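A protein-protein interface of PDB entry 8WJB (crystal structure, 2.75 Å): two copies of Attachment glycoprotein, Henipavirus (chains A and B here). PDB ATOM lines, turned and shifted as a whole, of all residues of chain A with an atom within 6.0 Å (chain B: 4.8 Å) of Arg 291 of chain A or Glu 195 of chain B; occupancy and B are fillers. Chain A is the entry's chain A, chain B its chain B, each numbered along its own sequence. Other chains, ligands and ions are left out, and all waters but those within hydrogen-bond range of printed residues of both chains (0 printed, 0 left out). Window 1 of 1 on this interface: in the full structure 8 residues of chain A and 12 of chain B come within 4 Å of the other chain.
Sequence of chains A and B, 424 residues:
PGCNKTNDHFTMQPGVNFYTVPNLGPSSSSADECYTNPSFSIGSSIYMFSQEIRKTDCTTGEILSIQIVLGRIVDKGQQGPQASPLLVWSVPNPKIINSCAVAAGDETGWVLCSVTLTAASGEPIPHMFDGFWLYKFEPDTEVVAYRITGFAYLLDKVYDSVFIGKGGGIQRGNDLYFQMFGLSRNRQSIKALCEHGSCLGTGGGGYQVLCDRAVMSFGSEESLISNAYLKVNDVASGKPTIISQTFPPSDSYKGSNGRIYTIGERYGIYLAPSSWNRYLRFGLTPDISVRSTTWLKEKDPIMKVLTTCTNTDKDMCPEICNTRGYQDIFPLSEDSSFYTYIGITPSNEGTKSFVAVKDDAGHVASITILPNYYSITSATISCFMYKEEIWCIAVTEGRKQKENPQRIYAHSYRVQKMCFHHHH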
ATOM      1  N   GLN A 245       5.917  17.289 -14.670  1.00  0.00           N
ATOM      2  CA  GLN A 245       5.489  18.553 -14.088  1.00  0.00           C
ATOM      3  C   GLN A 245       5.473  19.600 -15.203  1.00  0.00           C
ATOM      4  O   GLN A 245       6.524  19.970 -15.749  1.00  0.00           O
ATOM      5  CB  GLN A 245       6.393  18.948 -12.932  1.00  0.00           C
ATOM      6  CG  GLN A 245       5.722  19.787 -11.884  1.00  0.00           C
ATOM      7  CD  GLN A 245       6.598  19.924 -10.665  1.00  0.00           C
ATOM      8  OE1 GLN A 245       7.565  19.172 -10.494  1.00  0.00           O
ATOM      9  NE2 GLN A 245       6.288  20.898  -9.817  1.00  0.00           N
ATOM     10  N   ASP A 251       4.714  30.784 -17.046  1.00  0.00           N
ATOM     11  CA  ASP A 251       6.134  30.594 -16.799  1.00  0.00           C
ATOM     12  C   ASP A 251       6.864  30.031 -18.019  1.00  0.00           C
ATOM     13  O   ASP A 251       7.993  29.544 -17.888  1.00  0.00           O
ATOM     14  CB  ASP A 251       6.330  29.705 -15.564  1.00  0.00           C
ATOM     15  CG  ASP A 251       7.580  30.082 -14.751  1.00  0.00           C
ATOM     16  OD1 ASP A 251       8.063  31.248 -14.851  1.00  0.00           O
ATOM     17  OD2 ASP A 251       8.077  29.202 -14.000  1.00  0.00           O
ATOM     18  N   THR A 285      17.480  25.419 -11.374  1.00  0.00           N
ATOM     19  CA  THR A 285      16.576  24.938 -10.343  1.00  0.00           C
ATOM     20  C   THR A 285      17.300  23.997  -9.384  1.00  0.00           C
ATOM     21  O   THR A 285      17.948  23.028  -9.806  1.00  0.00           O
ATOM     22  CB  THR A 285      15.339  24.296 -10.984  1.00  0.00           C
ATOM     23  OG1 THR A 285      14.386  23.997  -9.962  1.00  0.00           O
ATOM     24  CG2 THR A 285      15.675  23.043 -11.784  1.00  0.00           C
ATOM     25  N   SER A 289      11.632  21.331 -10.529  1.00  0.00           N
ATOM     26  CA  SER A 289      10.244  21.625 -10.195  1.00  0.00           C
ATOM     27  C   SER A 289       9.874  23.011 -10.705  1.00  0.00           C
ATOM     28  O   SER A 289      10.698  23.930 -10.696  1.00  0.00           O
ATOM     29  CB  SER A 289       9.996  21.542  -8.690  1.00  0.00           C
ATOM     30  OG  SER A 289      10.441  22.710  -8.038  1.00  0.00           O
ATOM     31  N   VAL A 290       8.621  23.156 -11.139  1.00  0.00           N
ATOM     32  CA  VAL A 290       8.234  24.384 -11.816  1.00  0.00           C
ATOM     33  C   VAL A 290       8.266  25.566 -10.865  1.00  0.00           C
ATOM     34  O   VAL A 290       8.488  26.712 -11.283  1.00  0.00           O
ATOM     35  CB  VAL A 290       6.863  24.195 -12.474  1.00  0.00           C
ATOM     36  CG1 VAL A 290       6.285  25.514 -12.900  1.00  0.00           C
ATOM     37  CG2 VAL A 290       7.039  23.330 -13.676  1.00  0.00           C
ATOM     38  N   ARG A 291       8.085  25.320  -9.577  1.00  0.00           N
ATOM     39  CA  ARG A 291       8.053  26.432  -8.644  1.00  0.00           C
ATOM     40  C   ARG A 291       9.453  26.943  -8.317  1.00  0.00           C
ATOM     41  O   ARG A 291       9.643  28.156  -8.174  1.00  0.00           O
ATOM     42  CB  ARG A 291       7.298  26.017  -7.380  1.00  0.00           C
ATOM     43  CG  ARG A 291       6.919  27.171  -6.520  1.00  0.00           C
ATOM     44  CD  ARG A 291       6.189  26.789  -5.273  1.00  0.00           C
ATOM     45  NE  ARG A 291       5.969  28.009  -4.507  1.00  0.00           N
ATOM     46  CZ  ARG A 291       5.285  28.100  -3.377  1.00  0.00           C
ATOM     47  NH1 ARG A 291       4.744  27.035  -2.809  1.00  0.00           N
ATOM     48  NH2 ARG A 291       5.136  29.292  -2.807  1.00  0.00           N
ATOM     49  N   SER A 292      10.452  26.065  -8.249  1.00  0.00           N
ATOM     50  CA  SER A 292      11.807  26.475  -7.895  1.00  0.00           C
ATOM     51  C   SER A 292      12.661  26.864  -9.108  1.00  0.00           C
ATOM     52  O   SER A 292      13.863  27.101  -8.954  1.00  0.00           O
ATOM     53  CB  SER A 292      12.496  25.358  -7.120  1.00  0.00           C
ATOM     54  OG  SER A 292      12.855  24.304  -7.997  1.00  0.00           O
ATOM     55  N   THR A 293      12.068  26.963 -10.295  1.00  0.00           N
ATOM     56  CA  THR A 293      12.798  27.259 -11.524  1.00  0.00           C
ATOM     57  C   THR A 293      12.926  28.767 -11.694  1.00  0.00           C
ATOM     58  O   THR A 293      11.914  29.473 -11.782  1.00  0.00           O
ATOM     59  CB  THR A 293      12.071  26.675 -12.734  1.00  0.00           C
ATOM     60  OG1 THR A 293      11.851  25.272 -12.535  1.00  0.00           O
ATOM     61  CG2 THR A 293      12.887  26.913 -14.014  1.00  0.00           C
ATOM     62  N   THR A 294      14.156  29.249 -11.769  1.00  0.00           N
ATOM     63  CA  THR A 294      14.466  30.658 -11.951  1.00  0.00           C
ATOM     64  C   THR A 294      15.097  30.840 -13.316  1.00  0.00           C
ATOM     65  O   THR A 294      15.946  30.042 -13.716  1.00  0.00           O
ATOM     66  CB  THR A 294      15.452  31.127 -10.889  1.00  0.00           C
ATOM     67  OG1 THR A 294      14.843  30.998  -9.605  1.00  0.00           O
ATOM     68  CG2 THR A 294      15.845  32.573 -11.126  1.00  0.00           C
ATOM     69  N   LEU B 193      -5.192  20.615  -4.788  1.00  0.00           N
ATOM     70  CA  LEU B 193      -3.839  21.048  -5.109  1.00  0.00           C
ATOM     71  C   LEU B 193      -2.792  20.226  -4.360  1.00  0.00           C
ATOM     72  O   LEU B 193      -2.825  20.131  -3.131  1.00  0.00           O
ATOM     73  CB  LEU B 193      -3.688  22.527  -4.780  1.00  0.00           C
ATOM     74  CG  LEU B 193      -2.404  23.138  -5.322  1.00  0.00           C
ATOM     75  CD1 LEU B 193      -2.132  22.618  -6.752  1.00  0.00           C
ATOM     76  CD2 LEU B 193      -2.474  24.663  -5.257  1.00  0.00           C
ATOM     77  N   CYS B 194      -1.849  19.643  -5.101  1.00  0.00           N
ATOM     78  CA  CYS B 194      -0.882  18.703  -4.530  1.00  0.00           C
ATOM     79  C   CYS B 194       0.539  19.029  -5.007  1.00  0.00           C
ATOM     80  O   CYS B 194       1.304  18.154  -5.424  1.00  0.00           O
ATOM     81  CB  CYS B 194      -1.284  17.263  -4.877  1.00  0.00           C
ATOM     82  SG  CYS B 194      -1.127  16.029  -3.529  1.00  0.00           S
ATOM     83  N   GLU B 195       0.915  20.307  -4.932  1.00  0.00           N
ATOM     84  CA  GLU B 195       2.228  20.761  -5.379  1.00  0.00           C
ATOM     85  C   GLU B 195       3.240  20.647  -4.241  1.00  0.00           C
ATOM     86  O   GLU B 195       3.135  21.359  -3.233  1.00  0.00           O
ATOM     87  CB  GLU B 195       2.165  22.198  -5.892  1.00  0.00           C
ATOM     88  CG  GLU B 195       3.503  22.689  -6.441  1.00  0.00           C
ATOM     89  CD  GLU B 195       3.460  24.144  -6.873  1.00  0.00           C
ATOM     90  OE1 GLU B 195       2.546  24.865  -6.407  1.00  0.00           O
ATOM     91  OE2 GLU B 195       4.338  24.556  -7.673  1.00  0.00           O
ATOM     92  N   HIS B 196       4.234  19.785  -4.420  1.00  0.00           N
ATOM     93  CA  HIS B 196       5.222  19.503  -3.384  1.00  0.00           C
ATOM     94  C   HIS B 196       6.579  19.340  -4.048  1.00  0.00           C
ATOM     95  O   HIS B 196       6.800  19.761  -5.187  1.00  0.00           O
ATOM     96  CB  HIS B 196       4.830  18.248  -2.595  1.00  0.00           C
ATOM     97  CG  HIS B 196       4.411  17.106  -3.461  1.00  0.00           C
ATOM     98  ND1 HIS B 196       5.317  16.340  -4.161  1.00  0.00           N
ATOM     99  CD2 HIS B 196       3.188  16.613  -3.755  1.00  0.00           C
ATOM    100  CE1 HIS B 196       4.668  15.413  -4.842  1.00  0.00           C
ATOM    101  NE2 HIS B 196       3.375  15.558  -4.612  1.00  0.00           N
ATOM    102  N   GLY B 197       7.497  18.719  -3.324  1.00  0.00           N
ATOM    103  CA  GLY B 197       8.848  18.510  -3.790  1.00  0.00           C
ATOM    104  C   GLY B 197       9.082  17.047  -4.066  1.00  0.00           C
ATOM    105  O   GLY B 197       8.149  16.338  -4.457  1.00  0.00           O
ATOM    106  N   TYR B 253      -5.399  25.118  -0.985  1.00  0.00           N
ATOM    107  CA  TYR B 253      -5.201  24.097   0.033  1.00  0.00           C
ATOM    108  C   TYR B 253      -6.330  24.182   1.065  1.00  0.00           C
ATOM    109  O   TYR B 253      -7.374  24.795   0.817  1.00  0.00           O
ATOM    110  CB  TYR B 253      -3.812  24.255   0.659  1.00  0.00           C
ATOM    111  CG  TYR B 253      -2.695  24.133  -0.342  1.00  0.00           C
ATOM    112  CD1 TYR B 253      -2.311  22.889  -0.843  1.00  0.00           C
ATOM    113  CD2 TYR B 253      -2.022  25.252  -0.789  1.00  0.00           C
ATOM    114  CE1 TYR B 253      -1.297  22.771  -1.782  1.00  0.00           C
ATOM    115  CE2 TYR B 253      -1.002  25.148  -1.715  1.00  0.00           C
ATOM    116  CZ  TYR B 253      -0.640  23.905  -2.211  1.00  0.00           C
ATOM    117  OH  TYR B 253       0.383  23.820  -3.137  1.00  0.00           O
ATOM    118  N   TRP B 276      -0.634  20.844   5.235  1.00  0.00           N
ATOM    119  CA  TRP B 276       0.713  20.346   4.988  1.00  0.00           C
ATOM    120  C   TRP B 276       1.577  21.352   4.231  1.00  0.00           C
ATOM    121  O   TRP B 276       2.801  21.297   4.336  1.00  0.00           O
ATOM    122  CB  TRP B 276       0.646  19.018   4.225  1.00  0.00           C
ATOM    123  CG  TRP B 276      -0.021  19.176   2.900  1.00  0.00           C
ATOM    124  CD1 TRP B 276      -1.342  19.032   2.636  1.00  0.00           C
ATOM    125  CD2 TRP B 276       0.599  19.565   1.660  1.00  0.00           C
ATOM    126  NE1 TRP B 276      -1.592  19.274   1.305  1.00  0.00           N
ATOM    127  CE2 TRP B 276      -0.419  19.611   0.684  1.00  0.00           C
ATOM    128  CE3 TRP B 276       1.916  19.874   1.280  1.00  0.00           C
ATOM    129  CZ2 TRP B 276      -0.167  19.945  -0.644  1.00  0.00           C
ATOM    130  CZ3 TRP B 276       2.165  20.211  -0.047  1.00  0.00           C
ATOM    131  CH2 TRP B 276       1.129  20.244  -0.988  1.00  0.00           C
ATOM    132  N   ASN B 277       0.977  22.249   3.448  1.00  0.00           N
ATOM    133  CA  ASN B 277       1.759  23.261   2.681  1.00  0.00           C
ATOM    134  C   ASN B 277       2.047  24.464   3.578  1.00  0.00           C
ATOM    135  O   ASN B 277       1.108  25.223   3.856  1.00  0.00           O
ATOM    136  CB  ASN B 277       1.107  23.672   1.363  1.00  0.00           C
ATOM    137  CG  ASN B 277       2.040  24.455   0.468  1.00  0.00           C
ATOM    138  OD1 ASN B 277       2.247  25.645   0.675  1.00  0.00           O
ATOM    139  ND2 ASN B 277       2.597  23.798  -0.533  1.00  0.00           N
ATOM    140  N   TYR B 279       4.283  26.773   3.092  1.00  0.00           N
ATOM    141  CA  TYR B 279       4.940  27.866   2.344  1.00  0.00           C
ATOM    142  C   TYR B 279       4.065  29.101   2.228  1.00  0.00           C
ATOM    143  O   TYR B 279       3.094  29.251   2.987  1.00  0.00           O
ATOM    144  CB  TYR B 279       5.171  27.530   0.877  1.00  0.00           C
ATOM    145  CG  TYR B 279       6.133  26.402   0.689  1.00  0.00           C
ATOM    146  CD1 TYR B 279       7.362  26.424   1.322  1.00  0.00           C
ATOM    147  CD2 TYR B 279       5.801  25.310  -0.085  1.00  0.00           C
ATOM    148  CE1 TYR B 279       8.244  25.377   1.174  1.00  0.00           C
ATOM    149  CE2 TYR B 279       6.677  24.254  -0.243  1.00  0.00           C
ATOM    150  CZ  TYR B 279       7.905  24.288   0.393  1.00  0.00           C
ATOM    151  OH  TYR B 279       8.807  23.276   0.285  1.00  0.00           O
ATOM    152  N   LEU B 280       4.475  29.986   1.329  1.00  0.00           N
ATOM    153  CA  LEU B 280       3.740  31.256   1.147  1.00  0.00           C
ATOM    154  C   LEU B 280       2.603  31.055   0.143  1.00  0.00           C
ATOM    155  O   LEU B 280       2.849  30.578  -0.975  1.00  0.00           O
ATOM    156  CB  LEU B 280       4.725  32.353   0.716  1.00  0.00           C
ATOM    157  CG  LEU B 280       4.112  33.698   0.353  1.00  0.00           C
ATOM    158  CD1 LEU B 280       3.340  34.282   1.526  1.00  0.00           C
ATOM    159  CD2 LEU B 280       5.190  34.664  -0.110  1.00  0.00           C
ATOM    160  N   LEU B 296       2.068  33.620  -6.188  1.00  0.00           N
ATOM    161  CA  LEU B 296       3.498  33.875  -6.256  1.00  0.00           C
ATOM    162  C   LEU B 296       4.267  32.558  -6.202  1.00  0.00           C
ATOM    163  O   LEU B 296       3.795  31.558  -5.658  1.00  0.00           O
ATOM    164  CB  LEU B 296       3.933  34.808  -5.113  1.00  0.00           C
ATOM    165  CG  LEU B 296       3.468  36.274  -5.189  1.00  0.00           C
ATOM    166  CD1 LEU B 296       4.136  37.141  -4.101  1.00  0.00           C
ATOM    167  CD2 LEU B 296       3.680  36.873  -6.590  1.00  0.00           C
ATOM    168  N   LYS B 297       5.457  32.550  -6.798  1.00  0.00           N
ATOM    169  CA  LYS B 297       6.265  31.342  -6.759  1.00  0.00           C
ATOM    170  C   LYS B 297       7.116  31.252  -5.506  1.00  0.00           C
ATOM    171  O   LYS B 297       7.473  30.143  -5.103  1.00  0.00           O
ATOM    172  CB  LYS B 297       7.157  31.244  -8.007  1.00  0.00           C
ATOM    173  CG  LYS B 297       6.453  30.647  -9.231  1.00  0.00           C
ATOM    174  CD  LYS B 297       7.329  30.683 -10.463  1.00  0.00           C
ATOM    175  CE  LYS B 297       8.807  30.558 -10.098  1.00  0.00           C
ATOM    176  NZ  LYS B 297       9.678  30.590 -11.327  1.00  0.00           N
ATOM    177  N   GLU B 298       7.415  32.377  -4.867  1.00  0.00           N
ATOM    178  CA  GLU B 298       8.382  32.398  -3.774  1.00  0.00           C
ATOM    179  C   GLU B 298       7.803  31.738  -2.528  1.00  0.00           C
ATOM    180  O   GLU B 298       6.607  31.818  -2.260  1.00  0.00           O
ATOM    181  CB  GLU B 298       8.816  33.840  -3.480  1.00  0.00           C
ATOM    182  CG  GLU B 298       9.902  33.921  -2.433  1.00  0.00           C
ATOM    183  CD  GLU B 298      11.306  33.690  -2.987  1.00  0.00           C
ATOM    184  OE1 GLU B 298      11.633  34.170  -4.105  1.00  0.00           O
ATOM    185  OE2 GLU B 298      12.085  33.001  -2.292  1.00  0.00           O
ATOM    186  N   LYS B 299       8.658  31.066  -1.765  1.00  0.00           N
ATOM    187  CA  LYS B 299       8.174  30.270  -0.642  1.00  0.00           C
ATOM    188  C   LYS B 299       8.311  30.941   0.726  1.00  0.00           C
ATOM    189  O   LYS B 299       7.749  30.412   1.695  1.00  0.00           O
ATOM    190  CB  LYS B 299       8.874  28.902  -0.618  1.00  0.00           C
ATOM    191  CG  LYS B 299       8.818  28.167  -1.940  1.00  0.00           C
ATOM    192  CD  LYS B 299       9.516  26.828  -1.856  1.00  0.00           C
ATOM    193  CE  LYS B 299       9.747  26.226  -3.225  1.00  0.00           C
ATOM    194  NZ  LYS B 299      10.553  24.998  -3.098  1.00  0.00           N
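The guanidinium group (NH2) of Arg 291 of chain A sits at hydrogen-bond distance from the backbone carbonyl oxygen (O) of Leu 280 of chain B. The backbone carbonyl oxygen (O) of Lys 297 of chain B sits at hydrogen-bond distance from the guanidinium group (NE) of Arg 291 of chain A, 2.7 Å away. NH2 of Arg 291 of chain A sits at hydrogen-bond distance from O of Glu 298 of chain B (3.0 Å). The side-chain amino group (NZ) of Lys 297 of chain B sits at hydrogen-bond distance from the backbone carbonyl oxygen (O) of Thr 293 of chain A, at 2.5 Å. OD2 of Asp 251 of chain A is in salt-bridge range of NZ of Lys 297 of chain B (3.4 Å).
OD1 of Asn 277 of chain B lies close to N of Tyr 279 of chain B (3.4 Å). The backbone carbonyl oxygen (O) of Ser 289 of chain A is in hydrogen-bond range of the side-chain hydroxyl (OG1) of Thr 293 of chain A, at 2.6 Å. O of Lys 299 of chain B lies within hydrogen-bond range of N of Leu 280 of chain B (3.3 Å).
CB of Arg 291 of chain A touches OE2 of Glu 195 of chain B, 3.3 Å away. Arg 291 of chain A touches Tyr 279 of chain B. Arg 291 of chain A touches Leu 296 of chain B. CG of Lys 299 of chain B touches CZ of Arg 291 of chain A, 3.8 Å away.
Arg 291 of chain A touches seven residues of chain B. Printed residues of chain A within 4 Å of Glu 195 of chain B: Arg 291. Printed residues of chain A within 4 Å of Lys 297 of chain B: Asp 251 (3.4 Å), Arg 291 (2.7 Å) and Thr 293 (2.5 Å). Of the printed residues of chain A, Lys 299 of chain B touches Arg 291 (3.8 Å). Gln 245 of chain A touches none of the printed residues of chain B. The nearest residue of chain B that does not touch Arg 291 of chain A is Asn 277 of chain B (4.5 Å). The nearest printed residue of chain B that does not touch Asp 251 of chain A is Glu 195 of chain B (8.7 Å).
Along chain B the printed residues that touch a printed residue of chain A span positions 195 to 299. Among the printed residues, Asp or Glu carboxylates within 4 Å of a Lys or Arg side-chain nitrogen of the other chain: Asp 251 of chain A with Lys 297 of chain B.
No position is printed for both chains.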
